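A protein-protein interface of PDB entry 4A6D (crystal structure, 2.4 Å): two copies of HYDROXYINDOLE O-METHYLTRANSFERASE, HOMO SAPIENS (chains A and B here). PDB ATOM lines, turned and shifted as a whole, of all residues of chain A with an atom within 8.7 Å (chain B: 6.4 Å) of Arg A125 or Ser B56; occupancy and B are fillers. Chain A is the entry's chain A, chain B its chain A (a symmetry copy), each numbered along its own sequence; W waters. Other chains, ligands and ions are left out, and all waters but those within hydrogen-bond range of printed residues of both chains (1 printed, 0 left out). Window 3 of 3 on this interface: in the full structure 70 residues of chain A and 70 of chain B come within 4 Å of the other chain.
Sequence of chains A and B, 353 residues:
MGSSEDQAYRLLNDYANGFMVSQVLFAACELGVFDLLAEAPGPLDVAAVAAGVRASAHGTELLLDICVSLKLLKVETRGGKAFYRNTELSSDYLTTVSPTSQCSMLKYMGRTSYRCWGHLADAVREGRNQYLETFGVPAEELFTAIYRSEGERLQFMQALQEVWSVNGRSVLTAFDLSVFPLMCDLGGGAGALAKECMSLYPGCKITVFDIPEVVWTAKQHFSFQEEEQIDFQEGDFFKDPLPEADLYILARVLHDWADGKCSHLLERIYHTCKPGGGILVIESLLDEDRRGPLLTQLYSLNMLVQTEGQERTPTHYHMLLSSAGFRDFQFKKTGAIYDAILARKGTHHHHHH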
ATOM      1  N   GLY A 118      30.756 -19.654 -13.393  1.00  0.00           N
ATOM      2  CA  GLY A 118      29.961 -19.842 -12.185  1.00  0.00           C
ATOM      3  C   GLY A 118      28.743 -18.928 -12.206  1.00  0.00           C
ATOM      4  O   GLY A 118      27.699 -19.244 -11.632  1.00  0.00           O
ATOM      5  N   HIS A 119      28.861 -17.808 -12.931  1.00  0.00           N
ATOM      6  CA  HIS A 119      27.797 -16.823 -13.115  1.00  0.00           C
ATOM      7  C   HIS A 119      27.025 -17.052 -14.437  1.00  0.00           C
ATOM      8  O   HIS A 119      26.407 -16.110 -14.932  1.00  0.00           O
ATOM      9  CB  HIS A 119      28.369 -15.387 -13.047  1.00  0.00           C
ATOM     10  CG  HIS A 119      29.148 -15.117 -11.804  1.00  0.00           C
ATOM     11  ND1 HIS A 119      28.520 -14.812 -10.616  1.00  0.00           N
ATOM     12  CD2 HIS A 119      30.484 -15.142 -11.600  1.00  0.00           C
ATOM     13  CE1 HIS A 119      29.487 -14.665  -9.723  1.00  0.00           C
ATOM     14  NE2 HIS A 119      30.686 -14.847 -10.270  1.00  0.00           N
ATOM     15  N   LEU A 120      27.005 -18.307 -14.959  1.00  0.00           N
ATOM     16  CA  LEU A 120      26.330 -18.676 -16.217  1.00  0.00           C
ATOM     17  C   LEU A 120      24.837 -18.364 -16.216  1.00  0.00           C
ATOM     18  O   LEU A 120      24.340 -17.789 -17.192  1.00  0.00           O
ATOM     19  CB  LEU A 120      26.570 -20.153 -16.632  1.00  0.00           C
ATOM     20  CG  LEU A 120      25.867 -20.597 -17.930  1.00  0.00           C
ATOM     21  CD1 LEU A 120      26.350 -19.791 -19.137  1.00  0.00           C
ATOM     22  CD2 LEU A 120      26.054 -22.037 -18.194  1.00  0.00           C
ATOM     23  N   ALA A 121      24.135 -18.748 -15.141  1.00  0.00           N
ATOM     24  CA  ALA A 121      22.695 -18.553 -14.990  1.00  0.00           C
ATOM     25  C   ALA A 121      22.300 -17.083 -15.128  1.00  0.00           C
ATOM     26  O   ALA A 121      21.298 -16.797 -15.785  1.00  0.00           O
ATOM     27  CB  ALA A 121      22.211 -19.130 -13.668  1.00  0.00           C
ATOM     28  N   ASP A 122      23.128 -16.153 -14.602  1.00  0.00           N
ATOM     29  CA  ASP A 122      22.859 -14.724 -14.717  1.00  0.00           C
ATOM     30  C   ASP A 122      23.208 -14.174 -16.076  1.00  0.00           C
ATOM     31  O   ASP A 122      22.513 -13.277 -16.544  1.00  0.00           O
ATOM     32  CB  ASP A 122      23.529 -13.923 -13.601  1.00  0.00           C
ATOM     33  CG  ASP A 122      23.042 -14.237 -12.205  1.00  0.00           C
ATOM     34  OD1 ASP A 122      21.900 -14.769 -12.067  1.00  0.00           O
ATOM     35  OD2 ASP A 122      23.797 -13.974 -11.249  1.00  0.00           O
ATOM     36  N   ALA A 123      24.282 -14.692 -16.718  1.00  0.00           N
ATOM     37  CA  ALA A 123      24.684 -14.286 -18.078  1.00  0.00           C
ATOM     38  C   ALA A 123      23.584 -14.706 -19.053  1.00  0.00           C
ATOM     39  O   ALA A 123      23.241 -13.948 -19.934  1.00  0.00           O
ATOM     40  CB  ALA A 123      26.012 -14.912 -18.456  1.00  0.00           C
ATOM     41  N   VAL A 124      22.974 -15.870 -18.830  1.00  0.00           N
ATOM     42  CA  VAL A 124      21.826 -16.369 -19.590  1.00  0.00           C
ATOM     43  C   VAL A 124      20.613 -15.471 -19.238  1.00  0.00           C
ATOM     44  O   VAL A 124      20.012 -14.912 -20.150  1.00  0.00           O
ATOM     45  CB  VAL A 124      21.565 -17.885 -19.335  1.00  0.00           C
ATOM     46  CG1 VAL A 124      20.220 -18.330 -19.898  1.00  0.00           C
ATOM     47  CG2 VAL A 124      22.690 -18.742 -19.909  1.00  0.00           C
ATOM     48  N   ARG A 125      20.303 -15.305 -17.924  1.00  0.00           N
ATOM     49  CA  ARG A 125      19.212 -14.466 -17.409  1.00  0.00           C
ATOM     50  C   ARG A 125      19.208 -13.046 -17.982  1.00  0.00           C
ATOM     51  O   ARG A 125      18.166 -12.583 -18.432  1.00  0.00           O
ATOM     52  CB  ARG A 125      19.268 -14.377 -15.870  1.00  0.00           C
ATOM     53  CG  ARG A 125      18.241 -15.244 -15.164  1.00  0.00           C
ATOM     54  CD  ARG A 125      18.387 -15.210 -13.650  1.00  0.00           C
ATOM     55  NE  ARG A 125      17.729 -16.356 -13.030  1.00  0.00           N
ATOM     56  CZ  ARG A 125      18.356 -17.323 -12.362  1.00  0.00           C
ATOM     57  NH1 ARG A 125      19.675 -17.286 -12.206  1.00  0.00           N
ATOM     58  NH2 ARG A 125      17.664 -18.325 -11.820  1.00  0.00           N
ATOM     59  N   GLU A 126      20.368 -12.370 -17.978  1.00  0.00           N
ATOM     60  CA  GLU A 126      20.511 -10.974 -18.388  1.00  0.00           C
ATOM     61  C   GLU A 126      20.902 -10.749 -19.819  1.00  0.00           C
ATOM     62  O   GLU A 126      20.715  -9.635 -20.330  1.00  0.00           O
ATOM     63  CB  GLU A 126      21.500 -10.245 -17.457  1.00  0.00           C
ATOM     64  CG  GLU A 126      21.027 -10.138 -16.010  1.00  0.00           C
ATOM     65  CD  GLU A 126      22.115 -10.126 -14.950  1.00  0.00           C
ATOM     66  OE1 GLU A 126      23.152  -9.454 -15.164  1.00  0.00           O
ATOM     67  OE2 GLU A 126      21.916 -10.766 -13.890  1.00  0.00           O
ATOM     68  N   GLY A 127      21.504 -11.756 -20.442  1.00  0.00           N
ATOM     69  CA  GLY A 127      21.987 -11.658 -21.812  1.00  0.00           C
ATOM     70  C   GLY A 127      23.235 -10.809 -21.934  1.00  0.00           C
ATOM     71  O   GLY A 127      23.480 -10.220 -22.996  1.00  0.00           O
ATOM     72  N   ARG A 128      24.058 -10.770 -20.869  1.00  0.00           N
ATOM     73  CA  ARG A 128      25.292  -9.973 -20.870  1.00  0.00           C
ATOM     74  C   ARG A 128      26.462 -10.638 -20.111  1.00  0.00           C
ATOM     75  O   ARG A 128      26.229 -11.522 -19.283  1.00  0.00           O
ATOM     76  CB  ARG A 128      25.013  -8.529 -20.352  1.00  0.00           C
ATOM     77  CG  ARG A 128      24.626  -8.449 -18.871  1.00  0.00           C
ATOM     78  CD  ARG A 128      24.473  -7.024 -18.384  1.00  0.00           C
ATOM     79  NE  ARG A 128      23.068  -6.681 -18.153  1.00  0.00           N
ATOM     80  CZ  ARG A 128      22.549  -6.382 -16.967  1.00  0.00           C
ATOM     81  NH1 ARG A 128      23.317  -6.361 -15.884  1.00  0.00           N
ATOM     82  NH2 ARG A 128      21.260  -6.089 -16.856  1.00  0.00           N
ATOM     83  N   GLN A 130      29.822 -11.023 -17.431  1.00  0.00           N
ATOM     84  CA  GLN A 130      29.897 -10.893 -15.980  1.00  0.00           C
ATOM     85  C   GLN A 130      31.262 -10.502 -15.385  1.00  0.00           C
ATOM     86  O   GLN A 130      31.560 -10.920 -14.268  1.00  0.00           O
ATOM     87  CB  GLN A 130      29.365 -12.179 -15.301  1.00  0.00           C
ATOM     88  CG  GLN A 130      28.130 -12.807 -15.930  1.00  0.00           C
ATOM     89  CD  GLN A 130      26.882 -12.010 -15.687  1.00  0.00           C
ATOM     90  OE1 GLN A 130      26.492 -11.151 -16.478  1.00  0.00           O
ATOM     91  NE2 GLN A 130      26.211 -12.298 -14.603  1.00  0.00           N
ATOM     92  N   LEU A 301      28.428 -19.610 -26.116  1.00  0.00           N
ATOM     93  CA  LEU A 301      27.960 -19.364 -24.761  1.00  0.00           C
ATOM     94  C   LEU A 301      29.072 -18.723 -23.928  1.00  0.00           C
ATOM     95  O   LEU A 301      28.793 -17.784 -23.181  1.00  0.00           O
ATOM     96  CB  LEU A 301      27.400 -20.635 -24.135  1.00  0.00           C
ATOM     97  CG  LEU A 301      26.649 -20.480 -22.797  1.00  0.00           C
ATOM     98  CD1 LEU A 301      25.553 -19.402 -22.847  1.00  0.00           C
ATOM     99  CD2 LEU A 301      26.093 -21.794 -22.359  1.00  0.00           C
ATOM    100  N   LEU A 304      28.988 -15.065 -24.663  1.00  0.00           N
ATOM    101  CA  LEU A 304      27.903 -14.413 -23.944  1.00  0.00           C
ATOM    102  C   LEU A 304      28.366 -14.111 -22.508  1.00  0.00           C
ATOM    103  O   LEU A 304      28.204 -12.987 -22.037  1.00  0.00           O
ATOM    104  CB  LEU A 304      26.616 -15.277 -23.934  1.00  0.00           C
ATOM    105  CG  LEU A 304      25.478 -14.776 -23.020  1.00  0.00           C
ATOM    106  CD1 LEU A 304      24.896 -13.444 -23.526  1.00  0.00           C
ATOM    107  CD2 LEU A 304      24.391 -15.793 -22.893  1.00  0.00           C
ATOM    108  N   ALA B  27      22.872 -24.608 -14.667  1.00  0.00           N
ATOM    109  CA  ALA B  27      22.085 -23.421 -15.008  1.00  0.00           C
ATOM    110  C   ALA B  27      20.728 -23.797 -15.559  1.00  0.00           C
ATOM    111  O   ALA B  27      19.755 -23.128 -15.250  1.00  0.00           O
ATOM    112  CB  ALA B  27      22.834 -22.543 -15.995  1.00  0.00           C
ATOM    113  N   GLU B  30      18.951 -24.658 -12.337  1.00  0.00           N
ATOM    114  CA  GLU B  30      18.680 -23.413 -11.618  1.00  0.00           C
ATOM    115  C   GLU B  30      17.547 -22.592 -12.296  1.00  0.00           C
ATOM    116  O   GLU B  30      16.723 -22.010 -11.596  1.00  0.00           O
ATOM    117  CB  GLU B  30      19.981 -22.582 -11.426  1.00  0.00           C
ATOM    118  CG  GLU B  30      19.748 -21.133 -10.969  1.00  0.00           C
ATOM    119  CD  GLU B  30      20.730 -20.436 -10.038  1.00  0.00           C
ATOM    120  OE1 GLU B  30      21.394 -21.121  -9.229  1.00  0.00           O
ATOM    121  OE2 GLU B  30      20.786 -19.185 -10.078  1.00  0.00           O
ATOM    122  N   LEU B  31      17.494 -22.567 -13.646  1.00  0.00           N
ATOM    123  CA  LEU B  31      16.466 -21.813 -14.375  1.00  0.00           C
ATOM    124  C   LEU B  31      15.095 -22.504 -14.455  1.00  0.00           C
ATOM    125  O   LEU B  31      14.097 -21.848 -14.758  1.00  0.00           O
ATOM    126  CB  LEU B  31      16.961 -21.384 -15.750  1.00  0.00           C
ATOM    127  CG  LEU B  31      17.988 -20.277 -15.762  1.00  0.00           C
ATOM    128  CD1 LEU B  31      18.864 -20.384 -16.989  1.00  0.00           C
ATOM    129  CD2 LEU B  31      17.323 -18.917 -15.716  1.00  0.00           C
ATOM    130  N   VAL B  46      11.789 -21.339 -28.187  1.00  0.00           N
ATOM    131  CA  VAL B  46      12.753 -20.475 -27.469  1.00  0.00           C
ATOM    132  C   VAL B  46      12.046 -19.343 -26.697  1.00  0.00           C
ATOM    133  O   VAL B  46      12.264 -19.198 -25.495  1.00  0.00           O
ATOM    134  CB  VAL B  46      13.896 -19.935 -28.400  1.00  0.00           C
ATOM    135  CG1 VAL B  46      14.823 -18.960 -27.665  1.00  0.00           C
ATOM    136  CG2 VAL B  46      14.707 -21.076 -29.008  1.00  0.00           C
ATOM    137  N   ALA B  50      12.225 -18.864 -22.749  1.00  0.00           N
ATOM    138  CA  ALA B  50      12.808 -17.589 -22.303  1.00  0.00           C
ATOM    139  C   ALA B  50      11.858 -16.784 -21.412  1.00  0.00           C
ATOM    140  O   ALA B  50      12.302 -16.226 -20.408  1.00  0.00           O
ATOM    141  CB  ALA B  50      13.240 -16.753 -23.494  1.00  0.00           C
ATOM    142  N   VAL B  53      11.201 -18.966 -17.934  1.00  0.00           N
ATOM    143  CA  VAL B  53      12.371 -19.001 -17.043  1.00  0.00           C
ATOM    144  C   VAL B  53      12.858 -17.587 -16.683  1.00  0.00           C
ATOM    145  O   VAL B  53      13.724 -17.436 -15.815  1.00  0.00           O
ATOM    146  CB  VAL B  53      13.524 -19.930 -17.527  1.00  0.00           C
ATOM    147  CG1 VAL B  53      13.054 -21.372 -17.652  1.00  0.00           C
ATOM    148  CG2 VAL B  53      14.153 -19.445 -18.833  1.00  0.00           C
ATOM    149  N   ARG B  54      12.275 -16.559 -17.345  1.00  0.00           N
ATOM    150  CA  ARG B  54      12.587 -15.136 -17.187  1.00  0.00           C
ATOM    151  C   ARG B  54      14.056 -14.863 -17.497  1.00  0.00           C
ATOM    152  O   ARG B  54      14.830 -14.443 -16.637  1.00  0.00           O
ATOM    153  CB  ARG B  54      12.093 -14.581 -15.834  1.00  0.00           C
ATOM    154  CG  ARG B  54      10.624 -14.177 -15.900  1.00  0.00           C
ATOM    155  CD  ARG B  54       9.899 -14.281 -14.574  1.00  0.00           C
ATOM    156  NE  ARG B  54       9.424 -15.638 -14.291  1.00  0.00           N
ATOM    157  CZ  ARG B  54       8.229 -16.113 -14.638  1.00  0.00           C
ATOM    158  NH1 ARG B  54       7.375 -15.354 -15.321  1.00  0.00           N
ATOM    159  NH2 ARG B  54       7.883 -17.354 -14.315  1.00  0.00           N
ATOM    160  N   ALA B  55      14.431 -15.152 -18.755  1.00  0.00           N
ATOM    161  CA  ALA B  55      15.788 -15.035 -19.273  1.00  0.00           C
ATOM    162  C   ALA B  55      15.799 -14.494 -20.701  1.00  0.00           C
ATOM    163  O   ALA B  55      14.746 -14.363 -21.332  1.00  0.00           O
ATOM    164  CB  ALA B  55      16.477 -16.395 -19.211  1.00  0.00           C
ATOM    165  N   SER B  56      16.998 -14.159 -21.197  1.00  0.00           N
ATOM    166  CA  SER B  56      17.201 -13.598 -22.522  1.00  0.00           C
ATOM    167  C   SER B  56      17.034 -14.638 -23.620  1.00  0.00           C
ATOM    168  O   SER B  56      17.353 -15.808 -23.419  1.00  0.00           O
ATOM    169  CB  SER B  56      18.575 -12.938 -22.613  1.00  0.00           C
ATOM    170  OG  SER B  56      19.634 -13.881 -22.642  1.00  0.00           O
ATOM    171  N   ALA B  57      16.557 -14.182 -24.787  1.00  0.00           N
ATOM    172  CA  ALA B  57      16.333 -14.952 -26.009  1.00  0.00           C
ATOM    173  C   ALA B  57      17.616 -15.637 -26.455  1.00  0.00           C
ATOM    174  O   ALA B  57      17.635 -16.869 -26.572  1.00  0.00           O
ATOM    175  CB  ALA B  57      15.819 -14.034 -27.108  1.00  0.00           C
ATOM    176  N   HIS B  58      18.699 -14.849 -26.652  1.00  0.00           N
ATOM    177  CA  HIS B  58      19.998 -15.374 -27.066  1.00  0.00           C
ATOM    178  C   HIS B  58      20.524 -16.432 -26.097  1.00  0.00           C
ATOM    179  O   HIS B  58      20.863 -17.536 -26.528  1.00  0.00           O
ATOM    180  CB  HIS B  58      21.020 -14.246 -27.305  1.00  0.00           C
ATOM    181  CG  HIS B  58      22.303 -14.729 -27.920  1.00  0.00           C
ATOM    182  ND1 HIS B  58      22.322 -15.378 -29.152  1.00  0.00           N
ATOM    183  CD2 HIS B  58      23.568 -14.670 -27.441  1.00  0.00           C
ATOM    184  CE1 HIS B  58      23.590 -15.691 -29.373  1.00  0.00           C
ATOM    185  NE2 HIS B  58      24.376 -15.279 -28.375  1.00  0.00           N
ATOM    186  N   GLY B  59      20.498 -16.110 -24.803  1.00  0.00           N
ATOM    187  CA  GLY B  59      20.940 -16.987 -23.723  1.00  0.00           C
ATOM    188  C   GLY B  59      20.181 -18.290 -23.635  1.00  0.00           C
ATOM    189  O   GLY B  59      20.797 -19.356 -23.520  1.00  0.00           O
ATOM    190  N   THR B  60      18.834 -18.214 -23.710  1.00  0.00           N
ATOM    191  CA  THR B  60      17.945 -19.380 -23.654  1.00  0.00           C
ATOM    192  C   THR B  60      18.217 -20.324 -24.821  1.00  0.00           C
ATOM    193  O   THR B  60      18.377 -21.518 -24.582  1.00  0.00           O
ATOM    194  CB  THR B  60      16.473 -18.945 -23.583  1.00  0.00           C
ATOM    195  OG1 THR B  60      16.289 -18.105 -22.445  1.00  0.00           O
ATOM    196  CG2 THR B  60      15.523 -20.108 -23.500  1.00  0.00           C
ATOM    197  N   GLU B  61      18.301 -19.785 -26.070  1.00  0.00           N
ATOM    198  CA  GLU B  61      18.549 -20.581 -27.268  1.00  0.00           C
ATOM    199  C   GLU B  61      19.877 -21.299 -27.186  1.00  0.00           C
ATOM    200  O   GLU B  61      19.938 -22.492 -27.475  1.00  0.00           O
ATOM    201  CB  GLU B  61      18.455 -19.743 -28.544  1.00  0.00           C
ATOM    202  CG  GLU B  61      18.362 -20.609 -29.791  1.00  0.00           C
ATOM    203  CD  GLU B  61      18.788 -19.997 -31.113  1.00  0.00           C
ATOM    204  OE1 GLU B  61      19.827 -19.296 -31.158  1.00  0.00           O
ATOM    205  OE2 GLU B  61      18.125 -20.309 -32.128  1.00  0.00           O
ATOM    206  N   ARG B 111      26.504 -24.369  -7.075  1.00  0.00           N
ATOM    207  CA  ARG B 111      26.629 -23.249  -6.135  1.00  0.00           C
ATOM    208  C   ARG B 111      27.793 -23.361  -5.141  1.00  0.00           C
ATOM    209  O   ARG B 111      28.348 -22.338  -4.767  1.00  0.00           O
ATOM    210  CB  ARG B 111      25.289 -23.006  -5.389  1.00  0.00           C
ATOM    211  CG  ARG B 111      24.162 -22.489  -6.300  1.00  0.00           C
ATOM    212  CD  ARG B 111      22.753 -22.747  -5.776  1.00  0.00           C
ATOM    213  NE  ARG B 111      21.749 -22.576  -6.836  1.00  0.00           N
ATOM    214  CZ  ARG B 111      20.465 -22.910  -6.729  1.00  0.00           C
ATOM    215  NH1 ARG B 111      20.000 -23.442  -5.605  1.00  0.00           N
ATOM    216  NH2 ARG B 111      19.635 -22.717  -7.749  1.00  0.00           N
HETATM  217  O   HOH W   1      26.905 -15.345 -27.374  1.00  0.00           O
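Arg A125 touches just these residues of chain B: Glu B30, Leu B31, Arg B54, Ala B55 and Ser B56. Of chain A, only Val A124, Arg A125 and Gly A127 come within 4 Å of Ser B56. Ala B55 touches two residues of chain A. Printed residues of chain A within 4 Å of Leu B31: Val A124 (3.8 Å) and Arg A125 (3.7 Å). Of the printed residues of chain A, Ala B27 touches Leu A120. Of the printed residues of chain B, Val A124 touches Leu B31, Ala B55, Ser B56 and Gly B59. Of the printed residues of chain B, Ala A121 touches Glu B30. Leu A301 touches none of the printed residues of chain B. The nearest printed residue of chain A that does not touch Ala B27 is Ala A121 (4.1 Å).
O of Val A124 is in hydrogen-bond range of OG of Ser B56, at 2.7 Å. The guanidinium group of Arg A125 lies within salt-bridge range of the side-chain carboxylate of Glu B30 (3.1 Å). The backbone carbonyl oxygen (O) of Arg A125 is in hydrogen-bond range of the backbone NH (N) of Ser B56, 3.4 Å away.
Printed residues of chain A that touch a printed residue of chain B: Leu A120, Ala A121, Val A124, Arg A125, Gly A127 and Leu A304. Hydrophobic or aromatic side chains of chain A that line the printed part of chain B: Leu A120, Ala A121, Val A124 and Leu A304. Printed residues of chain B that touch a printed residue of chain A: Ala B27, Glu B30, Leu B31, Arg B54, Ala B55, Ser B56 and Gly B59. Among the printed residues, 13 pairs touch across the chains.
Water W1 lies within hydrogen-bond range of a ring nitrogen (NE2) of His B58 (2.7 Å) and the backbone NH of Leu A304 (3.4 Å).
OD1 of Asp A122 is in salt-bridge range of NH1 of Arg A125 (3.4 Å). The side-chain carboxylate (OE1) of Glu B30 is in salt-bridge range of the guanidinium group (NH2) of Arg B111 (2.8 Å). The backbone carbonyl oxygen of Ala B50 is in hydrogen-bond range of the backbone NH of Ala B55, 2.9 Å away. The side-chain hydroxyl (OG) of Ser B56 sits at hydrogen-bond distance from the backbone NH (N) of Gly B59, 3.2 Å away. The backbone carbonyl oxygen (O) of Ser B56 is in hydrogen-bond range of the side-chain hydroxyl (OG1) of Thr B60, 2.7 Å away.
No position is printed for both chains. Of the 13 pairs that touch across the chains among the printed residues, none has its exchanged pair printed and touching as well.
Ala B27 touches Leu A120 (CB to CD2, 3.9 Å). Ala A121 touches Glu B30 (CB to OE2, 3.9 Å). CD1 of Leu B31 touches CG1 of Val A124, at 3.8 Å. Ala B55 touches Val A124 (CB to O, 3.9 Å). Val A124 touches Gly B59. Leu B31 touches Arg A125. Arg A125 touches Arg B54. Ala B55 touches Arg A125. OG of Ser B56 touches CA of Gly A127 (3.3 Å). Gly B59 touches Leu A304.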
